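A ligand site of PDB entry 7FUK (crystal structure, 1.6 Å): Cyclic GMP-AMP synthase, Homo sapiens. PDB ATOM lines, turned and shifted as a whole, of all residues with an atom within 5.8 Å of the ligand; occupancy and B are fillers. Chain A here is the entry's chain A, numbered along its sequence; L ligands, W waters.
The backbone NH (N) of Phe 219 lies within hydrogen-bond range of an oxygen (O2) of the ligand (3.0 Å). The backbone NH (N) of Ser 220 sits at hydrogen-bond distance from an oxygen (O1) of the ligand, at 3.2 Å. The side-chain hydroxyl of Ser 218 lies within hydrogen-bond range of an oxygen (O1) of the ligand, 2.7 Å away.
The side-chain carboxylate (OE2) of Glu 223 is in salt-bridge range of the side-chain amino group (NZ) of Lys 279, at 2.9 Å. The backbone NH of Phe 324 sits at hydrogen-bond distance from the side-chain amide oxygen of Asn 322 (2.9 Å). OG1 of Thr 280 is in hydrogen-bond range of O of Tyr 276 (3.0 Å). SD of Met 69 lies close to OG of Ser 220 (3.5 Å). O of Tyr 323 sits at hydrogen-bond distance from N of Leu 178 (2.9 Å). ND2 of Asn 322 is in hydrogen-bond range of OH of Tyr 276, at 3.3 Å. The backbone carbonyl oxygen of Phe 283 sits at hydrogen-bond distance from the side-chain hydroxyl of Tyr 323 (3.2 Å). O of Val 200 lies within hydrogen-bond range of N of Arg 216, 2.9 Å away.
Residues that only touch the ligand: Thr 280 (3.2 Å), Val 200 (3.2 Å), Tyr 276 (3.3 Å), Arg 216 (3.4 Å), Phe 283 (3.4 Å), Glu 223 (3.4 Å), Phe 324 (3.5 Å), Lys 59 (3.5 Å), Ile 226 (3.7 Å), Tyr 323 (3.8 Å) and Ile 222 (3.8 Å). Within 4 Å of the ligand: Lys 59, Val 200, Arg 216, Ser 218, Phe 219, Ser 220, Ile 222, Glu 223, Ile 226, Tyr 276, Thr 280, Phe 283, Tyr 323 and Phe 324. The nearest printed residue that does not touch the ligand is Lys 279 (4.2 Å).
Water W3 lies within hydrogen-bond range of an oxygen (O2) of the ligand (2.6 Å), the side-chain hydroxyl (OH) of Tyr 276 (2.7 Å) and the side-chain amide oxygen (OD1) of Asn 322 (3.0 Å). Water W2 lies within hydrogen-bond range of an oxygen (O2) of the ligand (2.7 Å), the backbone carbonyl oxygen (O) of Leu 217 (2.8 Å) and the side-chain amide nitrogen (ND2) of Asn 322 (3.1 Å). Water W1 lies within hydrogen-bond range of a nitrogen (N2) of the ligand, the side-chain amino group of Lys 279 and the side-chain amino group of Lys 59.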
ATOM      1  N   LYS A  59      33.095  -0.980  24.097  1.00  0.00           N
ATOM      2  CA  LYS A  59      31.794  -0.439  24.487  1.00  0.00           C
ATOM      3  C   LYS A  59      31.291  -1.226  25.685  1.00  0.00           C
ATOM      4  O   LYS A  59      31.339  -2.463  25.695  1.00  0.00           O
ATOM      5  CB  LYS A  59      30.822  -0.541  23.318  1.00  0.00           C
ATOM      6  CG  LYS A  59      29.364  -0.313  23.666  1.00  0.00           C
ATOM      7  CD  LYS A  59      28.611   0.268  22.480  1.00  0.00           C
ATOM      8  CE  LYS A  59      28.676  -0.627  21.279  1.00  0.00           C
ATOM      9  NZ  LYS A  59      27.293  -0.996  20.837  1.00  0.00           N
ATOM     10  N   MET A  69      33.864  -4.957  18.439  1.00  0.00           N
ATOM     11  CA  MET A  69      33.536  -5.293  17.053  1.00  0.00           C
ATOM     12  C   MET A  69      34.814  -5.409  16.231  1.00  0.00           C
ATOM     13  O   MET A  69      35.615  -4.466  16.175  1.00  0.00           O
ATOM     14  CB  MET A  69      32.589  -4.248  16.447  1.00  0.00           C
ATOM     15  CG  MET A  69      31.891  -4.691  15.165  1.00  0.00           C
ATOM     16  SD  MET A  69      30.286  -3.877  14.923  1.00  0.00           S
ATOM     17  CE  MET A  69      29.557  -4.092  16.553  1.00  0.00           C
ATOM     18  N   LEU A 178      17.314   6.673  10.347  1.00  0.00           N
ATOM     19  CA  LEU A 178      18.151   7.768  10.847  1.00  0.00           C
ATOM     20  C   LEU A 178      17.432   9.102  10.664  1.00  0.00           C
ATOM     21  O   LEU A 178      17.919  10.025  10.001  1.00  0.00           O
ATOM     22  CB  LEU A 178      19.529   7.775  10.169  1.00  0.00           C
ATOM     23  CG  LEU A 178      20.616   8.666  10.791  1.00  0.00           C
ATOM     24  CD1 LEU A 178      20.993   8.257  12.208  1.00  0.00           C
ATOM     25  CD2 LEU A 178      21.894   8.681   9.912  1.00  0.00           C
ATOM     26  N   VAL A 200      26.804  -8.230   9.888  1.00  0.00           N
ATOM     27  CA  VAL A 200      27.192  -9.178  10.931  1.00  0.00           C
ATOM     28  C   VAL A 200      26.572 -10.534  10.622  1.00  0.00           C
ATOM     29  O   VAL A 200      25.377 -10.610  10.282  1.00  0.00           O
ATOM     30  CB  VAL A 200      26.782  -8.679  12.317  1.00  0.00           C
ATOM     31  CG1 VAL A 200      27.468  -7.362  12.593  1.00  0.00           C
ATOM     32  CG2 VAL A 200      25.307  -8.485  12.377  1.00  0.00           C
ATOM     33  N   ARG A 216      23.091  -9.507   8.858  1.00  0.00           N
ATOM     34  CA  ARG A 216      22.238  -8.394   9.263  1.00  0.00           C
ATOM     35  C   ARG A 216      22.984  -7.073   9.141  1.00  0.00           C
ATOM     36  O   ARG A 216      24.155  -6.975   9.524  1.00  0.00           O
ATOM     37  CB  ARG A 216      21.727  -8.557  10.697  1.00  0.00           C
ATOM     38  CG  ARG A 216      20.693  -7.485  11.076  1.00  0.00           C
ATOM     39  CD  ARG A 216      20.465  -7.308  12.571  1.00  0.00           C
ATOM     40  NE  ARG A 216      19.687  -8.402  13.159  1.00  0.00           N
ATOM     41  CZ  ARG A 216      18.989  -8.305  14.284  1.00  0.00           C
ATOM     42  NH1 ARG A 216      18.318  -9.350  14.744  1.00  0.00           N
ATOM     43  NH2 ARG A 216      18.962  -7.163  14.948  1.00  0.00           N
ATOM     44  N   LEU A 217      22.310  -6.054   8.611  1.00  0.00           N
ATOM     45  CA  LEU A 217      22.878  -4.710   8.584  1.00  0.00           C
ATOM     46  C   LEU A 217      23.159  -4.209   9.993  1.00  0.00           C
ATOM     47  O   LEU A 217      22.349  -4.381  10.902  1.00  0.00           O
ATOM     48  CB  LEU A 217      21.929  -3.733   7.902  1.00  0.00           C
ATOM     49  CG  LEU A 217      21.447  -4.052   6.493  1.00  0.00           C
ATOM     50  CD1 LEU A 217      20.667  -2.879   5.947  1.00  0.00           C
ATOM     51  CD2 LEU A 217      22.635  -4.348   5.605  1.00  0.00           C
ATOM     52  N   SER A 218      24.289  -3.542  10.158  1.00  0.00           N
ATOM     53  CA  SER A 218      24.681  -3.040  11.463  1.00  0.00           C
ATOM     54  C   SER A 218      25.205  -1.619  11.372  1.00  0.00           C
ATOM     55  O   SER A 218      26.022  -1.295  10.504  1.00  0.00           O
ATOM     56  CB  SER A 218      25.737  -3.953  12.095  1.00  0.00           C
ATOM     57  OG  SER A 218      26.129  -3.435  13.361  1.00  0.00           O
ATOM     58  N   PHE A 219      24.740  -0.762  12.274  1.00  0.00           N
ATOM     59  CA  PHE A 219      25.141   0.641  12.296  1.00  0.00           C
ATOM     60  C   PHE A 219      25.609   1.062  13.686  1.00  0.00           C
ATOM     61  O   PHE A 219      25.506   2.232  14.055  1.00  0.00           O
ATOM     62  CB  PHE A 219      23.999   1.526  11.827  1.00  0.00           C
ATOM     63  CG  PHE A 219      23.462   1.131  10.500  1.00  0.00           C
ATOM     64  CD1 PHE A 219      22.458   0.172  10.399  1.00  0.00           C
ATOM     65  CD2 PHE A 219      23.988   1.677   9.325  1.00  0.00           C
ATOM     66  CE1 PHE A 219      21.967  -0.214   9.174  1.00  0.00           C
ATOM     67  CE2 PHE A 219      23.514   1.289   8.081  1.00  0.00           C
ATOM     68  CZ  PHE A 219      22.501   0.339   7.999  1.00  0.00           C
ATOM     69  N   SER A 220      26.164   0.119  14.451  1.00  0.00           N
ATOM     70  CA  SER A 220      26.541   0.448  15.826  1.00  0.00           C
ATOM     71  C   SER A 220      27.612   1.526  15.883  1.00  0.00           C
ATOM     72  O   SER A 220      27.675   2.277  16.862  1.00  0.00           O
ATOM     73  CB  SER A 220      26.996  -0.810  16.560  1.00  0.00           C
ATOM     74  OG  SER A 220      28.208  -1.283  16.027  1.00  0.00           O
ATOM     75  N   HIS A 221      28.461   1.644  14.851  1.00  0.00           N
ATOM     76  CA  HIS A 221      29.495   2.677  14.822  1.00  0.00           C
ATOM     77  C   HIS A 221      28.939   4.097  14.763  1.00  0.00           C
ATOM     78  O   HIS A 221      29.689   5.059  14.993  1.00  0.00           O
ATOM     79  CB  HIS A 221      30.426   2.453  13.614  1.00  0.00           C
ATOM     80  CG  HIS A 221      29.731   2.572  12.290  1.00  0.00           C
ATOM     81  ND1 HIS A 221      28.599   1.837  11.990  1.00  0.00           N
ATOM     82  CD2 HIS A 221      30.005   3.308  11.198  1.00  0.00           C
ATOM     83  CE1 HIS A 221      28.204   2.132  10.764  1.00  0.00           C
ATOM     84  NE2 HIS A 221      29.035   3.025  10.263  1.00  0.00           N
ATOM     85  N   ILE A 222      27.659   4.270  14.417  1.00  0.00           N
ATOM     86  CA  ILE A 222      27.070   5.609  14.358  1.00  0.00           C
ATOM     87  C   ILE A 222      26.750   6.145  15.748  1.00  0.00           C
ATOM     88  O   ILE A 222      26.627   7.369  15.915  1.00  0.00           O
ATOM     89  CB  ILE A 222      25.832   5.620  13.442  1.00  0.00           C
ATOM     90  CG1 ILE A 222      26.187   5.106  12.048  1.00  0.00           C
ATOM     91  CG2 ILE A 222      25.118   7.017  13.403  1.00  0.00           C
ATOM     92  CD1 ILE A 222      27.203   5.957  11.289  1.00  0.00           C
ATOM     93  N   GLU A 223      26.627   5.283  16.757  1.00  0.00           N
ATOM     94  CA  GLU A 223      26.178   5.767  18.059  1.00  0.00           C
ATOM     95  C   GLU A 223      27.108   6.852  18.599  1.00  0.00           C
ATOM     96  O   GLU A 223      26.654   7.925  19.009  1.00  0.00           O
ATOM     97  CB  GLU A 223      26.080   4.618  19.069  1.00  0.00           C
ATOM     98  CG  GLU A 223      25.481   5.128  20.398  1.00  0.00           C
ATOM     99  CD  GLU A 223      25.400   4.090  21.510  1.00  0.00           C
ATOM    100  OE1 GLU A 223      24.867   4.450  22.592  1.00  0.00           O
ATOM    101  OE2 GLU A 223      25.853   2.941  21.323  1.00  0.00           O
ATOM    102  N   ILE A 226      26.839  10.413  17.348  1.00  0.00           N
ATOM    103  CA  ILE A 226      25.653  11.165  17.738  1.00  0.00           C
ATOM    104  C   ILE A 226      25.604  11.387  19.251  1.00  0.00           C
ATOM    105  O   ILE A 226      25.295  12.495  19.688  1.00  0.00           O
ATOM    106  CB  ILE A 226      24.386  10.461  17.227  1.00  0.00           C
ATOM    107  CG1 ILE A 226      24.272  10.656  15.711  1.00  0.00           C
ATOM    108  CG2 ILE A 226      23.161  10.987  17.953  1.00  0.00           C
ATOM    109  CD1 ILE A 226      23.027  10.090  15.101  1.00  0.00           C
ATOM    110  N   TYR A 276      20.715  -2.335  23.947  1.00  0.00           N
ATOM    111  CA  TYR A 276      20.380  -1.941  22.577  1.00  0.00           C
ATOM    112  C   TYR A 276      18.936  -1.472  22.465  1.00  0.00           C
ATOM    113  O   TYR A 276      18.646  -0.475  21.804  1.00  0.00           O
ATOM    114  CB  TYR A 276      20.655  -3.104  21.625  1.00  0.00           C
ATOM    115  CG  TYR A 276      20.222  -2.924  20.164  1.00  0.00           C
ATOM    116  CD1 TYR A 276      20.560  -1.786  19.424  1.00  0.00           C
ATOM    117  CD2 TYR A 276      19.523  -3.930  19.506  1.00  0.00           C
ATOM    118  CE1 TYR A 276      20.172  -1.656  18.074  1.00  0.00           C
ATOM    119  CE2 TYR A 276      19.141  -3.820  18.167  1.00  0.00           C
ATOM    120  CZ  TYR A 276      19.461  -2.679  17.460  1.00  0.00           C
ATOM    121  OH  TYR A 276      19.084  -2.617  16.145  1.00  0.00           O
ATOM    122  N   LYS A 279      18.662   1.974  24.137  1.00  0.00           N
ATOM    123  CA  LYS A 279      19.286   3.003  23.314  1.00  0.00           C
ATOM    124  C   LYS A 279      18.403   3.372  22.133  1.00  0.00           C
ATOM    125  O   LYS A 279      18.210   4.549  21.816  1.00  0.00           O
ATOM    126  CB  LYS A 279      20.666   2.556  22.806  1.00  0.00           C
ATOM    127  CG  LYS A 279      21.791   2.575  23.770  1.00  0.00           C
ATOM    128  CD  LYS A 279      22.966   1.853  23.140  1.00  0.00           C
ATOM    129  CE  LYS A 279      24.133   1.800  24.101  1.00  0.00           C
ATOM    130  NZ  LYS A 279      25.314   1.173  23.500  1.00  0.00           N
ATOM    131  N   THR A 280      17.866   2.357  21.441  1.00  0.00           N
ATOM    132  CA  THR A 280      16.977   2.616  20.306  1.00  0.00           C
ATOM    133  C   THR A 280      15.793   3.467  20.717  1.00  0.00           C
ATOM    134  O   THR A 280      15.450   4.448  20.034  1.00  0.00           O
ATOM    135  CB  THR A 280      16.520   1.284  19.696  1.00  0.00           C
ATOM    136  OG1 THR A 280      17.684   0.586  19.198  1.00  0.00           O
ATOM    137  CG2 THR A 280      15.519   1.516  18.560  1.00  0.00           C
ATOM    138  N   PHE A 283      16.931   7.166  21.421  1.00  0.00           N
ATOM    139  CA  PHE A 283      17.174   8.007  20.248  1.00  0.00           C
ATOM    140  C   PHE A 283      15.892   8.350  19.488  1.00  0.00           C
ATOM    141  O   PHE A 283      15.800   9.413  18.880  1.00  0.00           O
ATOM    142  CB  PHE A 283      18.221   7.323  19.348  1.00  0.00           C
ATOM    143  CG  PHE A 283      19.625   7.450  19.907  1.00  0.00           C
ATOM    144  CD1 PHE A 283      20.229   8.711  20.039  1.00  0.00           C
ATOM    145  CD2 PHE A 283      20.316   6.344  20.368  1.00  0.00           C
ATOM    146  CE1 PHE A 283      21.506   8.840  20.604  1.00  0.00           C
ATOM    147  CE2 PHE A 283      21.603   6.477  20.919  1.00  0.00           C
ATOM    148  CZ  PHE A 283      22.178   7.725  21.033  1.00  0.00           C
ATOM    149  N   ASN A 322      13.790  -0.525  14.548  1.00  0.00           N
ATOM    150  CA  ASN A 322      15.212  -0.284  14.320  1.00  0.00           C
ATOM    151  C   ASN A 322      15.431   1.159  13.872  1.00  0.00           C
ATOM    152  O   ASN A 322      14.768   1.655  12.950  1.00  0.00           O
ATOM    153  CB  ASN A 322      15.695  -1.286  13.262  1.00  0.00           C
ATOM    154  CG  ASN A 322      17.210  -1.289  13.062  1.00  0.00           C
ATOM    155  OD1 ASN A 322      17.821  -0.244  12.860  1.00  0.00           O
ATOM    156  ND2 ASN A 322      17.797  -2.479  13.059  1.00  0.00           N
ATOM    157  N   TYR A 323      16.359   1.867  14.547  1.00  0.00           N
ATOM    158  CA  TYR A 323      16.542   3.287  14.279  1.00  0.00           C
ATOM    159  C   TYR A 323      16.982   3.567  12.856  1.00  0.00           C
ATOM    160  O   TYR A 323      16.744   4.665  12.347  1.00  0.00           O
ATOM    161  CB  TYR A 323      17.591   3.877  15.250  1.00  0.00           C
ATOM    162  CG  TYR A 323      17.475   5.382  15.424  1.00  0.00           C
ATOM    163  CD1 TYR A 323      16.388   5.953  16.102  1.00  0.00           C
ATOM    164  CD2 TYR A 323      18.468   6.235  14.944  1.00  0.00           C
ATOM    165  CE1 TYR A 323      16.275   7.326  16.261  1.00  0.00           C
ATOM    166  CE2 TYR A 323      18.377   7.614  15.121  1.00  0.00           C
ATOM    167  CZ  TYR A 323      17.266   8.153  15.771  1.00  0.00           C
ATOM    168  OH  TYR A 323      17.148   9.530  15.958  1.00  0.00           O
ATOM    169  N   PHE A 324      17.609   2.593  12.220  1.00  0.00           N
ATOM    170  CA  PHE A 324      18.124   2.707  10.867  1.00  0.00           C
ATOM    171  C   PHE A 324      17.256   2.016   9.835  1.00  0.00           C
ATOM    172  O   PHE A 324      17.372   2.339   8.645  1.00  0.00           O
ATOM    173  CB  PHE A 324      19.551   2.129  10.819  1.00  0.00           C
ATOM    174  CG  PHE A 324      20.519   2.937  11.616  1.00  0.00           C
ATOM    175  CD1 PHE A 324      20.558   2.809  13.005  1.00  0.00           C
ATOM    176  CD2 PHE A 324      21.325   3.887  10.998  1.00  0.00           C
ATOM    177  CE1 PHE A 324      21.419   3.599  13.756  1.00  0.00           C
ATOM    178  CE2 PHE A 324      22.175   4.704  11.743  1.00  0.00           C
ATOM    179  CZ  PHE A 324      22.228   4.547  13.126  1.00  0.00           C
HETATM  180  C1  LIG L   1      24.018  -3.881  17.489  1.00  0.00           C
HETATM  181  C2  LIG L   1      22.702  -5.662  16.303  1.00  0.00           C
HETATM  182  C3  LIG L   1      22.303  -8.033  16.174  1.00  0.00           C
HETATM  183  C4  LIG L   1      22.841  -8.076  14.916  1.00  0.00           C
HETATM  184  C5  LIG L   1      23.317  -6.912  14.343  1.00  0.00           C
HETATM  185  C6  LIG L   1      23.241  -5.720  15.026  1.00  0.00           C
HETATM  186  C7  LIG L   1      24.046  -2.436  19.554  1.00  0.00           C
HETATM  187  C8  LIG L   1      22.649   2.804  17.225  1.00  0.00           C
HETATM  188  C9  LIG L   1      21.440   3.361  17.702  1.00  0.00           C
HETATM  189  C10 LIG L   1      21.132   4.685  17.521  1.00  0.00           C
HETATM  190  C11 LIG L   1      22.025   5.545  16.898  1.00  0.00           C
HETATM  191  C12 LIG L   1      23.226   5.010  16.424  1.00  0.00           C
HETATM  192  C13 LIG L   1      23.528   3.664  16.585  1.00  0.00           C
HETATM  193  C14 LIG L   1      21.708   7.007  16.737  1.00  0.00           C
HETATM  194  C15 LIG L   1      23.000   0.506  16.272  1.00  0.00           C
HETATM  195  C16 LIG L   1      22.635  -4.350  17.049  1.00  0.00           C
HETATM  196  C17 LIG L   1      22.232  -6.831  16.871  1.00  0.00           C
HETATM  197  C18 LIG L   1      22.984   1.366  17.378  1.00  0.00           C
HETATM  198  C19 LIG L   1      23.267   0.841  18.630  1.00  0.00           C
HETATM  199  C20 LIG L   1      23.567  -0.502  18.805  1.00  0.00           C
HETATM  200  C21 LIG L   1      23.582  -1.362  17.698  1.00  0.00           C
HETATM  201  C22 LIG L   1      23.284  -0.850  16.424  1.00  0.00           C
HETATM  202  C23 LIG L   1      23.295  -1.584  15.107  1.00  0.00           C
HETATM  203  N1  LIG L   1      23.929  -2.618  18.209  1.00  0.00           N
HETATM  204  N2  LIG L   1      23.868  -1.203  19.958  1.00  0.00           N
HETATM  205  O1  LIG L   1      24.258  -2.414  14.995  1.00  0.00           O
HETATM  206  O2  LIG L   1      22.507  -1.320  14.179  1.00  0.00           O
HETATM  207 CL1  LIG L   1      20.259   2.366  18.499  1.00  0.00          CL
HETATM  208  O   HOH W   1      24.465  -1.451  22.669  1.00  0.00           O
HETATM  209  O   HOH W   2      20.874  -3.071  12.844  1.00  0.00           O
HETATM  210  O   HOH W   3      20.085  -0.481  14.740  1.00  0.00           O
